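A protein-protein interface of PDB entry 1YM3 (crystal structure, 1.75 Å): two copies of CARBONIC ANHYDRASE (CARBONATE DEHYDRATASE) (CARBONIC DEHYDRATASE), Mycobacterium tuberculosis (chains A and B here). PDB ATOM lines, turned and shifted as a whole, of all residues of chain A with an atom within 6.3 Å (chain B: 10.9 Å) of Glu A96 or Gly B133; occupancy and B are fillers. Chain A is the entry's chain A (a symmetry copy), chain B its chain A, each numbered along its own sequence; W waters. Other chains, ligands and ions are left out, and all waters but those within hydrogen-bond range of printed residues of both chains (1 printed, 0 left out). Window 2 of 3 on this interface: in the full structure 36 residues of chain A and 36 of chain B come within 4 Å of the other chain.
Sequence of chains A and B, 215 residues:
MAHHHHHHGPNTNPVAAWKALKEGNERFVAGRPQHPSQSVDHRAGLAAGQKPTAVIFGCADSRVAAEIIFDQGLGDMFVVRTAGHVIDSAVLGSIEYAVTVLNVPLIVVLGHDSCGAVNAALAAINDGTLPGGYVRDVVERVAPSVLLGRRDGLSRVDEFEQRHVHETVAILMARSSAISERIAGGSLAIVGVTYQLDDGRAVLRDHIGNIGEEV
The backbone carbonyl oxygen (O) of Thr B82 is in hydrogen-bond range of the backbone NH (N) of Ala B60, at 3.0 Å. OG1 of Thr B82 is in hydrogen-bond range of O of Val B86, 2.8 Å away. The side-chain hydroxyl (OG1) of Thr A100 lies within hydrogen-bond range of the backbone carbonyl oxygen (O) of Glu A96 (2.9 Å). The side-chain carboxylate (OE1) of Glu A96 is in hydrogen-bond range of the side-chain hydroxyl (OG) of Ser A176 (2.6 Å). O of Tyr A97 is in hydrogen-bond range of N of Leu A102 (3.3 Å).
Among the printed residues, merely in contact across the chains: Leu A92 with Tyr B134, Gly A93 with Tyr B134, Gly A93 with Val B138, Ser A94 with Thr B82, Ser A94 with Val B138, Glu A96 with Gly B133, Tyr A97 with Ala B120, Tyr A97 with Val B135 and Thr A100 with Val B135.
No position is printed for both chains.
Of chain B, only Gly B133, Tyr B134 and Val B135 come within 4 Å of Glu A96. Gly B133 touches one residue of chain A. Leu A92 touches just one residue of chain B: Tyr B134 (3.6 Å). Of chain B, only Tyr B134 and Val B138 come within 4 Å of Gly A93. No residue of chain B comes within 4 Å of Ile A95. No residue of chain B comes within 4 Å of Ala A98. No residue of chain B comes within 4 Å of Val A99. Of chain B, only Val B135 comes within 4 Å of Thr A100. No residue of chain B comes within 4 Å of Ser A177. No residue of chain B comes within 4 Å of Ala A178. Of the printed residues of chain A, Val B135 touches Glu A96, Tyr A97 and Thr A100. Printed residues of chain A within 4 Å of Tyr B134: Leu A92, Gly A93, Glu A96 and Arg A175. Of the printed residues of chain A, Val B138 touches Gly A93 and Ser A94. Of the printed residues of chain A, Ala B120 touches Tyr A97. Printed residues of chain A within 4 Å of Ala B83: Ser A94. The nearest residue of chain B that does not touch Glu A96 is Gly B132 (4.1 Å). The nearest printed residue of chain A that does not touch Gly B133 is Gly A93 (6.4 Å).
Water W1 lies within hydrogen-bond range of the side-chain hydroxyl of Tyr B134 (2.6 Å) and the backbone carbonyl oxygen of Arg A175 (2.7 Å).
Of the 18 printed residues of chain B, 7 touch a printed residue of chain A. Hydrophobic or aromatic side chains of chain A that line the printed part of chain B: Leu A92 and Tyr A97.
The backbone NH (N) of Ala B83 is in hydrogen-bond range of the side-chain hydroxyl (OG) of Ser A94 (2.8 Å). OE2 of Glu A96 sits at hydrogen-bond distance from N of Tyr B134. The side-chain hydroxyl (OH) of Tyr B134 lies within hydrogen-bond range of the guanidinium group (NH2) of Arg A175, at 3.1 Å. The side-chain carboxylate of Glu A96 lies within hydrogen-bond range of the backbone NH of Val B135 (3.4 Å).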
ATOM      1  N   VAL A  91     -10.378  13.887 -15.351  1.00  0.00           N
ATOM      2  CA  VAL A  91     -11.250  13.018 -16.119  1.00  0.00           C
ATOM      3  C   VAL A  91     -11.301  13.488 -17.585  1.00  0.00           C
ATOM      4  O   VAL A  91     -11.109  12.710 -18.517  1.00  0.00           O
ATOM      5  CB  VAL A  91     -12.652  12.974 -15.456  1.00  0.00           C
ATOM      6  CG1 VAL A  91     -13.597  12.098 -16.223  1.00  0.00           C
ATOM      7  CG2 VAL A  91     -12.511  12.506 -14.015  1.00  0.00           C
ATOM      8  N   LEU A  92     -11.554  14.768 -17.791  1.00  0.00           N
ATOM      9  CA  LEU A  92     -11.629  15.320 -19.121  1.00  0.00           C
ATOM     10  C   LEU A  92     -10.338  15.160 -19.881  1.00  0.00           C
ATOM     11  O   LEU A  92     -10.337  14.750 -21.060  1.00  0.00           O
ATOM     12  CB  LEU A  92     -12.172  16.778 -19.085  1.00  0.00           C
ATOM     13  CG  LEU A  92     -12.669  17.369 -20.366  1.00  0.00           C
ATOM     14  CD1 LEU A  92     -13.636  16.527 -21.140  1.00  0.00           C
ATOM     15  CD2 LEU A  92     -13.251  18.767 -20.035  1.00  0.00           C
ATOM     16  N   GLY A  93      -9.215  15.492 -19.247  1.00  0.00           N
ATOM     17  CA  GLY A  93      -7.916  15.318 -19.847  1.00  0.00           C
ATOM     18  C   GLY A  93      -7.607  13.895 -20.198  1.00  0.00           C
ATOM     19  O   GLY A  93      -6.960  13.653 -21.183  1.00  0.00           O
ATOM     20  N   SER A  94      -8.083  12.931 -19.377  1.00  0.00           N
ATOM     21  CA  SER A  94      -7.905  11.537 -19.705  1.00  0.00           C
ATOM     22  C   SER A  94      -8.571  11.159 -21.036  1.00  0.00           C
ATOM     23  O   SER A  94      -7.954  10.501 -21.881  1.00  0.00           O
ATOM     24  CB  SER A  94      -8.439  10.632 -18.585  1.00  0.00           C
ATOM     25  OG  SER A  94      -7.650  10.758 -17.409  1.00  0.00           O
ATOM     26  N   ILE A  95      -9.823  11.585 -21.201  1.00  0.00           N
ATOM     27  CA  ILE A  95     -10.564  11.290 -22.412  1.00  0.00           C
ATOM     28  C   ILE A  95      -9.950  12.031 -23.636  1.00  0.00           C
ATOM     29  O   ILE A  95      -9.708  11.431 -24.696  1.00  0.00           O
ATOM     30  CB  ILE A  95     -12.080  11.568 -22.206  1.00  0.00           C
ATOM     31  CG1 ILE A  95     -12.661  10.722 -21.050  1.00  0.00           C
ATOM     32  CG2 ILE A  95     -12.839  11.419 -23.527  1.00  0.00           C
ATOM     33  CD1 ILE A  95     -14.061  11.120 -20.631  1.00  0.00           C
ATOM     34  N   GLU A  96      -9.558  13.303 -23.428  1.00  0.00           N
ATOM     35  CA  GLU A  96      -8.931  14.102 -24.462  1.00  0.00           C
ATOM     36  C   GLU A  96      -7.596  13.519 -24.896  1.00  0.00           C
ATOM     37  O   GLU A  96      -7.296  13.472 -26.077  1.00  0.00           O
ATOM     38  CB  GLU A  96      -8.754  15.556 -23.982  1.00  0.00           C
ATOM     39  CG  GLU A  96      -8.736  16.579 -25.065  1.00  0.00           C
ATOM     40  CD  GLU A  96      -8.771  17.977 -24.484  1.00  0.00           C
ATOM     41  OE1 GLU A  96      -9.847  18.591 -24.279  1.00  0.00           O
ATOM     42  OE2 GLU A  96      -7.678  18.419 -24.246  1.00  0.00           O
ATOM     43  N   TYR A  97      -6.844  12.979 -23.944  1.00  0.00           N
ATOM     44  CA  TYR A  97      -5.605  12.275 -24.249  1.00  0.00           C
ATOM     45  C   TYR A  97      -5.813  11.077 -25.178  1.00  0.00           C
ATOM     46  O   TYR A  97      -5.067  10.905 -26.158  1.00  0.00           O
ATOM     47  CB  TYR A  97      -4.911  11.888 -22.940  1.00  0.00           C
ATOM     48  CG  TYR A  97      -3.749  10.917 -23.087  1.00  0.00           C
ATOM     49  CD1 TYR A  97      -2.460  11.363 -23.312  1.00  0.00           C
ATOM     50  CD2 TYR A  97      -3.964   9.545 -23.017  1.00  0.00           C
ATOM     51  CE1 TYR A  97      -1.426  10.469 -23.461  1.00  0.00           C
ATOM     52  CE2 TYR A  97      -2.959   8.656 -23.163  1.00  0.00           C
ATOM     53  CZ  TYR A  97      -1.673   9.120 -23.350  1.00  0.00           C
ATOM     54  OH  TYR A  97      -0.642   8.252 -23.504  1.00  0.00           O
ATOM     55  N   ALA A  98      -6.835  10.259 -24.919  1.00  0.00           N
ATOM     56  CA  ALA A  98      -7.085   9.100 -25.771  1.00  0.00           C
ATOM     57  C   ALA A  98      -7.436   9.549 -27.193  1.00  0.00           C
ATOM     58  O   ALA A  98      -7.026   8.950 -28.168  1.00  0.00           O
ATOM     59  CB  ALA A  98      -8.226   8.263 -25.187  1.00  0.00           C
ATOM     60  N   VAL A  99      -8.193  10.629 -27.302  1.00  0.00           N
ATOM     61  CA  VAL A  99      -8.641  11.113 -28.603  1.00  0.00           C
ATOM     62  C   VAL A  99      -7.521  11.806 -29.403  1.00  0.00           C
ATOM     63  O   VAL A  99      -7.382  11.579 -30.602  1.00  0.00           O
ATOM     64  CB  VAL A  99      -9.852  12.076 -28.375  1.00  0.00           C
ATOM     65  CG1 VAL A  99     -10.053  13.014 -29.572  1.00  0.00           C
ATOM     66  CG2 VAL A  99     -11.072  11.250 -28.052  1.00  0.00           C
ATOM     67  N   THR A 100      -6.746  12.668 -28.751  1.00  0.00           N
ATOM     68  CA  THR A 100      -5.752  13.493 -29.438  1.00  0.00           C
ATOM     69  C   THR A 100      -4.387  12.822 -29.573  1.00  0.00           C
ATOM     70  O   THR A 100      -3.685  13.050 -30.555  1.00  0.00           O
ATOM     71  CB  THR A 100      -5.570  14.866 -28.751  1.00  0.00           C
ATOM     72  OG1 THR A 100      -5.027  14.694 -27.432  1.00  0.00           O
ATOM     73  CG2 THR A 100      -6.899  15.608 -28.587  1.00  0.00           C
ATOM     74  N   VAL A 101      -3.963  12.093 -28.557  1.00  0.00           N
ATOM     75  CA  VAL A 101      -2.677  11.403 -28.568  1.00  0.00           C
ATOM     76  C   VAL A 101      -2.792  10.013 -29.142  1.00  0.00           C
ATOM     77  O   VAL A 101      -1.991   9.615 -29.996  1.00  0.00           O
ATOM     78  CB  VAL A 101      -2.030  11.415 -27.158  1.00  0.00           C
ATOM     79  CG1 VAL A 101      -0.695  10.672 -27.134  1.00  0.00           C
ATOM     80  CG2 VAL A 101      -1.845  12.858 -26.719  1.00  0.00           C
ATOM     81  N   LEU A 102      -3.798   9.259 -28.703  1.00  0.00           N
ATOM     82  CA  LEU A 102      -3.898   7.869 -29.132  1.00  0.00           C
ATOM     83  C   LEU A 102      -4.804   7.728 -30.382  1.00  0.00           C
ATOM     84  O   LEU A 102      -4.945   6.649 -30.907  1.00  0.00           O
ATOM     85  CB  LEU A 102      -4.386   6.972 -28.000  1.00  0.00           C
ATOM     86  CG  LEU A 102      -3.485   6.962 -26.762  1.00  0.00           C
ATOM     87  CD1 LEU A 102      -4.115   6.070 -25.716  1.00  0.00           C
ATOM     88  CD2 LEU A 102      -2.037   6.516 -27.060  1.00  0.00           C
ATOM     89  N   ARG A 175     -17.405  21.071 -23.049  1.00  0.00           N
ATOM     90  CA  ARG A 175     -16.215  21.436 -22.269  1.00  0.00           C
ATOM     91  C   ARG A 175     -14.887  21.237 -22.985  1.00  0.00           C
ATOM     92  O   ARG A 175     -13.900  21.866 -22.587  1.00  0.00           O
ATOM     93  CB  ARG A 175     -16.178  20.694 -20.936  1.00  0.00           C
ATOM     94  CG  ARG A 175     -17.307  21.084 -20.013  1.00  0.00           C
ATOM     95  CD  ARG A 175     -16.970  21.856 -18.747  1.00  0.00           C
ATOM     96  NE  ARG A 175     -15.565  21.901 -18.303  1.00  0.00           N
ATOM     97  CZ  ARG A 175     -15.082  21.412 -17.154  1.00  0.00           C
ATOM     98  NH1 ARG A 175     -15.855  20.775 -16.274  1.00  0.00           N
ATOM     99  NH2 ARG A 175     -13.796  21.573 -16.869  1.00  0.00           N
ATOM    100  N   SER A 176     -14.865  20.430 -24.046  1.00  0.00           N
ATOM    101  CA  SER A 176     -13.625  20.112 -24.771  1.00  0.00           C
ATOM    102  C   SER A 176     -13.692  20.462 -26.237  1.00  0.00           C
ATOM    103  O   SER A 176     -14.356  19.805 -27.033  1.00  0.00           O
ATOM    104  CB  SER A 176     -13.303  18.627 -24.623  1.00  0.00           C
ATOM    105  OG  SER A 176     -12.184  18.248 -25.399  1.00  0.00           O
ATOM    106  N   SER A 177     -13.002  21.533 -26.621  1.00  0.00           N
ATOM    107  CA  SER A 177     -12.979  21.884 -28.021  1.00  0.00           C
ATOM    108  C   SER A 177     -12.308  20.789 -28.855  1.00  0.00           C
ATOM    109  O   SER A 177     -12.648  20.629 -30.039  1.00  0.00           O
ATOM    110  CB  SER A 177     -12.309  23.260 -28.263  1.00  0.00           C
ATOM    111  OG  SER A 177     -10.970  23.279 -27.812  1.00  0.00           O
ATOM    112  N   ALA A 178     -11.340  20.074 -28.291  1.00  0.00           N
ATOM    113  CA  ALA A 178     -10.631  19.045 -29.057  1.00  0.00           C
ATOM    114  C   ALA A 178     -11.601  17.918 -29.443  1.00  0.00           C
ATOM    115  O   ALA A 178     -11.551  17.388 -30.567  1.00  0.00           O
ATOM    116  CB  ALA A 178      -9.465  18.479 -28.225  1.00  0.00           C
ATOM    117  N   ILE A 179     -12.497  17.580 -28.526  1.00  0.00           N
ATOM    118  CA  ILE A 179     -13.511  16.541 -28.761  1.00  0.00           C
ATOM    119  C   ILE A 179     -14.536  17.044 -29.799  1.00  0.00           C
ATOM    120  O   ILE A 179     -14.841  16.375 -30.798  1.00  0.00           O
ATOM    121  CB  ILE A 179     -14.213  16.134 -27.430  1.00  0.00           C
ATOM    122  CG1 ILE A 179     -13.226  15.323 -26.596  1.00  0.00           C
ATOM    123  CG2 ILE A 179     -15.521  15.379 -27.666  1.00  0.00           C
ATOM    124  CD1 ILE A 179     -13.626  14.925 -25.157  1.00  0.00           C
ATOM    125  N   ALA B  60      -6.069   4.292 -16.958  1.00  0.00           N
ATOM    126  CA  ALA B  60      -6.996   4.155 -18.069  1.00  0.00           C
ATOM    127  C   ALA B  60      -6.393   3.402 -19.223  1.00  0.00           C
ATOM    128  O   ALA B  60      -7.141   2.785 -20.019  1.00  0.00           O
ATOM    129  CB  ALA B  60      -7.523   5.526 -18.537  1.00  0.00           C
ATOM    130  N   THR B  82      -8.131   6.675 -14.193  1.00  0.00           N
ATOM    131  CA  THR B  82      -7.787   7.870 -14.995  1.00  0.00           C
ATOM    132  C   THR B  82      -6.451   7.634 -15.681  1.00  0.00           C
ATOM    133  O   THR B  82      -5.692   6.742 -15.285  1.00  0.00           O
ATOM    134  CB  THR B  82      -7.690   9.176 -14.117  1.00  0.00           C
ATOM    135  OG1 THR B  82      -6.644   9.022 -13.123  1.00  0.00           O
ATOM    136  CG2 THR B  82      -8.957   9.528 -13.441  1.00  0.00           C
ATOM    137  N   ALA B  83      -6.138   8.455 -16.688  1.00  0.00           N
ATOM    138  CA  ALA B  83      -4.855   8.340 -17.382  1.00  0.00           C
ATOM    139  C   ALA B  83      -3.707   8.676 -16.440  1.00  0.00           C
ATOM    140  O   ALA B  83      -3.680   9.739 -15.845  1.00  0.00           O
ATOM    141  CB  ALA B  83      -4.809   9.236 -18.624  1.00  0.00           C
ATOM    142  N   VAL B  86      -3.943  10.151 -12.507  1.00  0.00           N
ATOM    143  CA  VAL B  86      -4.063  11.551 -12.101  1.00  0.00           C
ATOM    144  C   VAL B  86      -5.308  11.793 -11.244  1.00  0.00           C
ATOM    145  O   VAL B  86      -6.365  11.209 -11.470  1.00  0.00           O
ATOM    146  CB  VAL B  86      -4.050  12.512 -13.306  1.00  0.00           C
ATOM    147  CG1 VAL B  86      -2.649  12.421 -13.922  1.00  0.00           C
ATOM    148  CG2 VAL B  86      -5.195  12.221 -14.338  1.00  0.00           C
ATOM    149  N   ALA B 120       4.334   9.527 -21.923  1.00  0.00           N
ATOM    150  CA  ALA B 120       3.938  10.837 -22.426  1.00  0.00           C
ATOM    151  C   ALA B 120       4.465  11.991 -21.542  1.00  0.00           C
ATOM    152  O   ALA B 120       4.919  13.033 -22.058  1.00  0.00           O
ATOM    153  CB  ALA B 120       2.391  10.909 -22.582  1.00  0.00           C
ATOM    154  N   THR B 129       7.954  21.739 -22.394  1.00  0.00           N
ATOM    155  CA  THR B 129       6.661  22.418 -22.454  1.00  0.00           C
ATOM    156  C   THR B 129       5.534  21.373 -22.377  1.00  0.00           C
ATOM    157  O   THR B 129       5.722  20.211 -22.737  1.00  0.00           O
ATOM    158  CB  THR B 129       6.568  23.351 -23.726  1.00  0.00           C
ATOM    159  OG1 THR B 129       7.339  24.567 -23.511  1.00  0.00           O
ATOM    160  CG2 THR B 129       5.147  23.878 -23.976  1.00  0.00           C
ATOM    161  N   LEU B 130       4.392  21.793 -21.855  1.00  0.00           N
ATOM    162  CA  LEU B 130       3.265  20.877 -21.644  1.00  0.00           C
ATOM    163  C   LEU B 130       2.312  20.897 -22.830  1.00  0.00           C
ATOM    164  O   LEU B 130       2.209  21.930 -23.490  1.00  0.00           O
ATOM    165  CB  LEU B 130       2.534  21.297 -20.368  1.00  0.00           C
ATOM    166  CG  LEU B 130       3.329  21.108 -19.076  1.00  0.00           C
ATOM    167  CD1 LEU B 130       2.631  21.856 -17.966  1.00  0.00           C
ATOM    168  CD2 LEU B 130       3.444  19.618 -18.723  1.00  0.00           C
ATOM    169  N   PRO B 131       1.579  19.798 -23.104  1.00  0.00           N
ATOM    170  CA  PRO B 131       0.589  19.785 -24.188  1.00  0.00           C
ATOM    171  C   PRO B 131      -0.597  20.662 -23.871  1.00  0.00           C
ATOM    172  O   PRO B 131      -0.717  21.199 -22.775  1.00  0.00           O
ATOM    173  CB  PRO B 131       0.156  18.307 -24.267  1.00  0.00           C
ATOM    174  CG  PRO B 131       0.365  17.825 -22.969  1.00  0.00           C
ATOM    175  CD  PRO B 131       1.639  18.492 -22.426  1.00  0.00           C
ATOM    176  N   GLY B 132      -1.485  20.814 -24.839  1.00  0.00           N
ATOM    177  CA  GLY B 132      -2.574  21.751 -24.713  1.00  0.00           C
ATOM    178  C   GLY B 132      -3.863  21.178 -24.187  1.00  0.00           C
ATOM    179  O   GLY B 132      -3.953  19.993 -23.831  1.00  0.00           O
ATOM    180  N   GLY B 133      -4.875  22.035 -24.129  1.00  0.00           N
ATOM    181  CA  GLY B 133      -6.185  21.653 -23.651  1.00  0.00           C
ATOM    182  C   GLY B 133      -6.105  21.009 -22.278  1.00  0.00           C
ATOM    183  O   GLY B 133      -5.316  21.421 -21.420  1.00  0.00           O
ATOM    184  N   TYR B 134      -6.959  19.994 -22.075  1.00  0.00           N
ATOM    185  CA  TYR B 134      -7.071  19.290 -20.811  1.00  0.00           C
ATOM    186  C   TYR B 134      -6.022  18.181 -20.731  1.00  0.00           C
ATOM    187  O   TYR B 134      -5.835  17.589 -19.689  1.00  0.00           O
ATOM    188  CB  TYR B 134      -8.535  18.752 -20.611  1.00  0.00           C
ATOM    189  CG  TYR B 134      -9.474  19.844 -20.137  1.00  0.00           C
ATOM    190  CD1 TYR B 134      -9.498  20.225 -18.804  1.00  0.00           C
ATOM    191  CD2 TYR B 134     -10.282  20.515 -21.024  1.00  0.00           C
ATOM    192  CE1 TYR B 134     -10.329  21.289 -18.372  1.00  0.00           C
ATOM    193  CE2 TYR B 134     -11.113  21.563 -20.612  1.00  0.00           C
ATOM    194  CZ  TYR B 134     -11.119  21.958 -19.279  1.00  0.00           C
ATOM    195  OH  TYR B 134     -11.961  23.000 -18.890  1.00  0.00           O
ATOM    196  N   VAL B 135      -5.327  17.897 -21.834  1.00  0.00           N
ATOM    197  CA  VAL B 135      -4.169  16.995 -21.761  1.00  0.00           C
ATOM    198  C   VAL B 135      -3.063  17.545 -20.872  1.00  0.00           C
ATOM    199  O   VAL B 135      -2.312  16.759 -20.253  1.00  0.00           O
ATOM    200  CB  VAL B 135      -3.637  16.615 -23.150  1.00  0.00           C
ATOM    201  CG1 VAL B 135      -2.539  15.586 -23.053  1.00  0.00           C
ATOM    202  CG2 VAL B 135      -4.796  16.064 -24.024  1.00  0.00           C
ATOM    203  N   ARG B 136      -2.942  18.875 -20.795  1.00  0.00           N
ATOM    204  CA  ARG B 136      -2.021  19.517 -19.859  1.00  0.00           C
ATOM    205  C   ARG B 136      -2.255  18.986 -18.432  1.00  0.00           C
ATOM    206  O   ARG B 136      -1.306  18.647 -17.692  1.00  0.00           O
ATOM    207  CB  ARG B 136      -2.200  21.033 -19.889  1.00  0.00           C
ATOM    208  CG  ARG B 136      -1.258  21.835 -18.944  1.00  0.00           C
ATOM    209  CD  ARG B 136      -1.694  23.297 -18.699  1.00  0.00           C
ATOM    210  NE  ARG B 136      -0.725  23.983 -17.836  1.00  0.00           N
ATOM    211  CZ  ARG B 136       0.407  24.536 -18.275  1.00  0.00           C
ATOM    212  NH1 ARG B 136       0.703  24.577 -19.576  1.00  0.00           N
ATOM    213  NH2 ARG B 136       1.231  25.103 -17.408  1.00  0.00           N
ATOM    214  N   ASP B 137      -3.523  18.920 -18.074  1.00  0.00           N
ATOM    215  CA  ASP B 137      -3.970  18.558 -16.722  1.00  0.00           C
ATOM    216  C   ASP B 137      -3.521  17.142 -16.331  1.00  0.00           C
ATOM    217  O   ASP B 137      -3.315  16.858 -15.143  1.00  0.00           O
ATOM    218  CB  ASP B 137      -5.488  18.699 -16.613  1.00  0.00           C
ATOM    219  CG  ASP B 137      -5.960  20.113 -16.913  1.00  0.00           C
ATOM    220  OD1 ASP B 137      -6.473  20.797 -15.992  1.00  0.00           O
ATOM    221  OD2 ASP B 137      -5.814  20.623 -18.046  1.00  0.00           O
ATOM    222  N   VAL B 138      -3.391  16.265 -17.315  1.00  0.00           N
ATOM    223  CA  VAL B 138      -2.879  14.908 -17.064  1.00  0.00           C
ATOM    224  C   VAL B 138      -1.353  14.949 -16.898  1.00  0.00           C
ATOM    225  O   VAL B 138      -0.771  14.550 -15.866  1.00  0.00           O
ATOM    226  CB  VAL B 138      -3.248  13.998 -18.216  1.00  0.00           C
ATOM    227  CG1 VAL B 138      -2.546  12.636 -18.086  1.00  0.00           C
ATOM    228  CG2 VAL B 138      -4.734  13.839 -18.265  1.00  0.00           C
ATOM    229  N   VAL B 139      -0.668  15.496 -17.899  1.00  0.00           N
ATOM    230  CA  VAL B 139       0.798  15.429 -17.879  1.00  0.00           C
ATOM    231  C   VAL B 139       1.391  16.187 -16.674  1.00  0.00           C
ATOM    232  O   VAL B 139       2.377  15.723 -16.082  1.00  0.00           O
ATOM    233  CB  VAL B 139       1.420  15.887 -19.227  1.00  0.00           C
ATOM    234  CG1 VAL B 139       2.929  15.997 -19.125  1.00  0.00           C
ATOM    235  CG2 VAL B 139       0.999  14.977 -20.349  1.00  0.00           C
ATOM    236  N   GLU B 140       0.774  17.292 -16.261  1.00  0.00           N
ATOM    237  CA  GLU B 140       1.292  18.091 -15.144  1.00  0.00           C
ATOM    238  C   GLU B 140       1.092  17.395 -13.778  1.00  0.00           C
ATOM    239  O   GLU B 140       1.662  17.796 -12.785  1.00  0.00           O
ATOM    240  CB  GLU B 140       0.693  19.525 -15.130  1.00  0.00           C
ATOM    241  CG  GLU B 140      -0.748  19.631 -14.645  1.00  0.00           C
ATOM    242  CD  GLU B 140      -1.359  21.027 -14.798  1.00  0.00           C
ATOM    243  OE1 GLU B 140      -0.591  22.028 -14.876  1.00  0.00           O
ATOM    244  OE2 GLU B 140      -2.622  21.112 -14.839  1.00  0.00           O
ATOM    245  N   ARG B 141       0.239  16.386 -13.730  1.00  0.00           N
ATOM    246  CA  ARG B 141      -0.011  15.648 -12.504  1.00  0.00           C
ATOM    247  C   ARG B 141       0.871  14.400 -12.487  1.00  0.00           C
ATOM    248  O   ARG B 141       1.049  13.832 -11.413  1.00  0.00           O
ATOM    249  CB  ARG B 141      -1.496  15.299 -12.359  1.00  0.00           C
ATOM    250  CG  ARG B 141      -2.386  16.500 -11.931  1.00  0.00           C
ATOM    251  CD  ARG B 141      -3.855  16.195 -12.029  1.00  0.00           C
ATOM    252  NE  ARG B 141      -4.702  17.239 -11.447  1.00  0.00           N
ATOM    253  CZ  ARG B 141      -4.971  18.419 -12.005  1.00  0.00           C
ATOM    254  NH1 ARG B 141      -4.407  18.778 -13.150  1.00  0.00           N
ATOM    255  NH2 ARG B 141      -5.774  19.274 -11.366  1.00  0.00           N
HETATM  256  O   HOH W   1     -14.030  23.438 -20.403  1.00  0.00           O
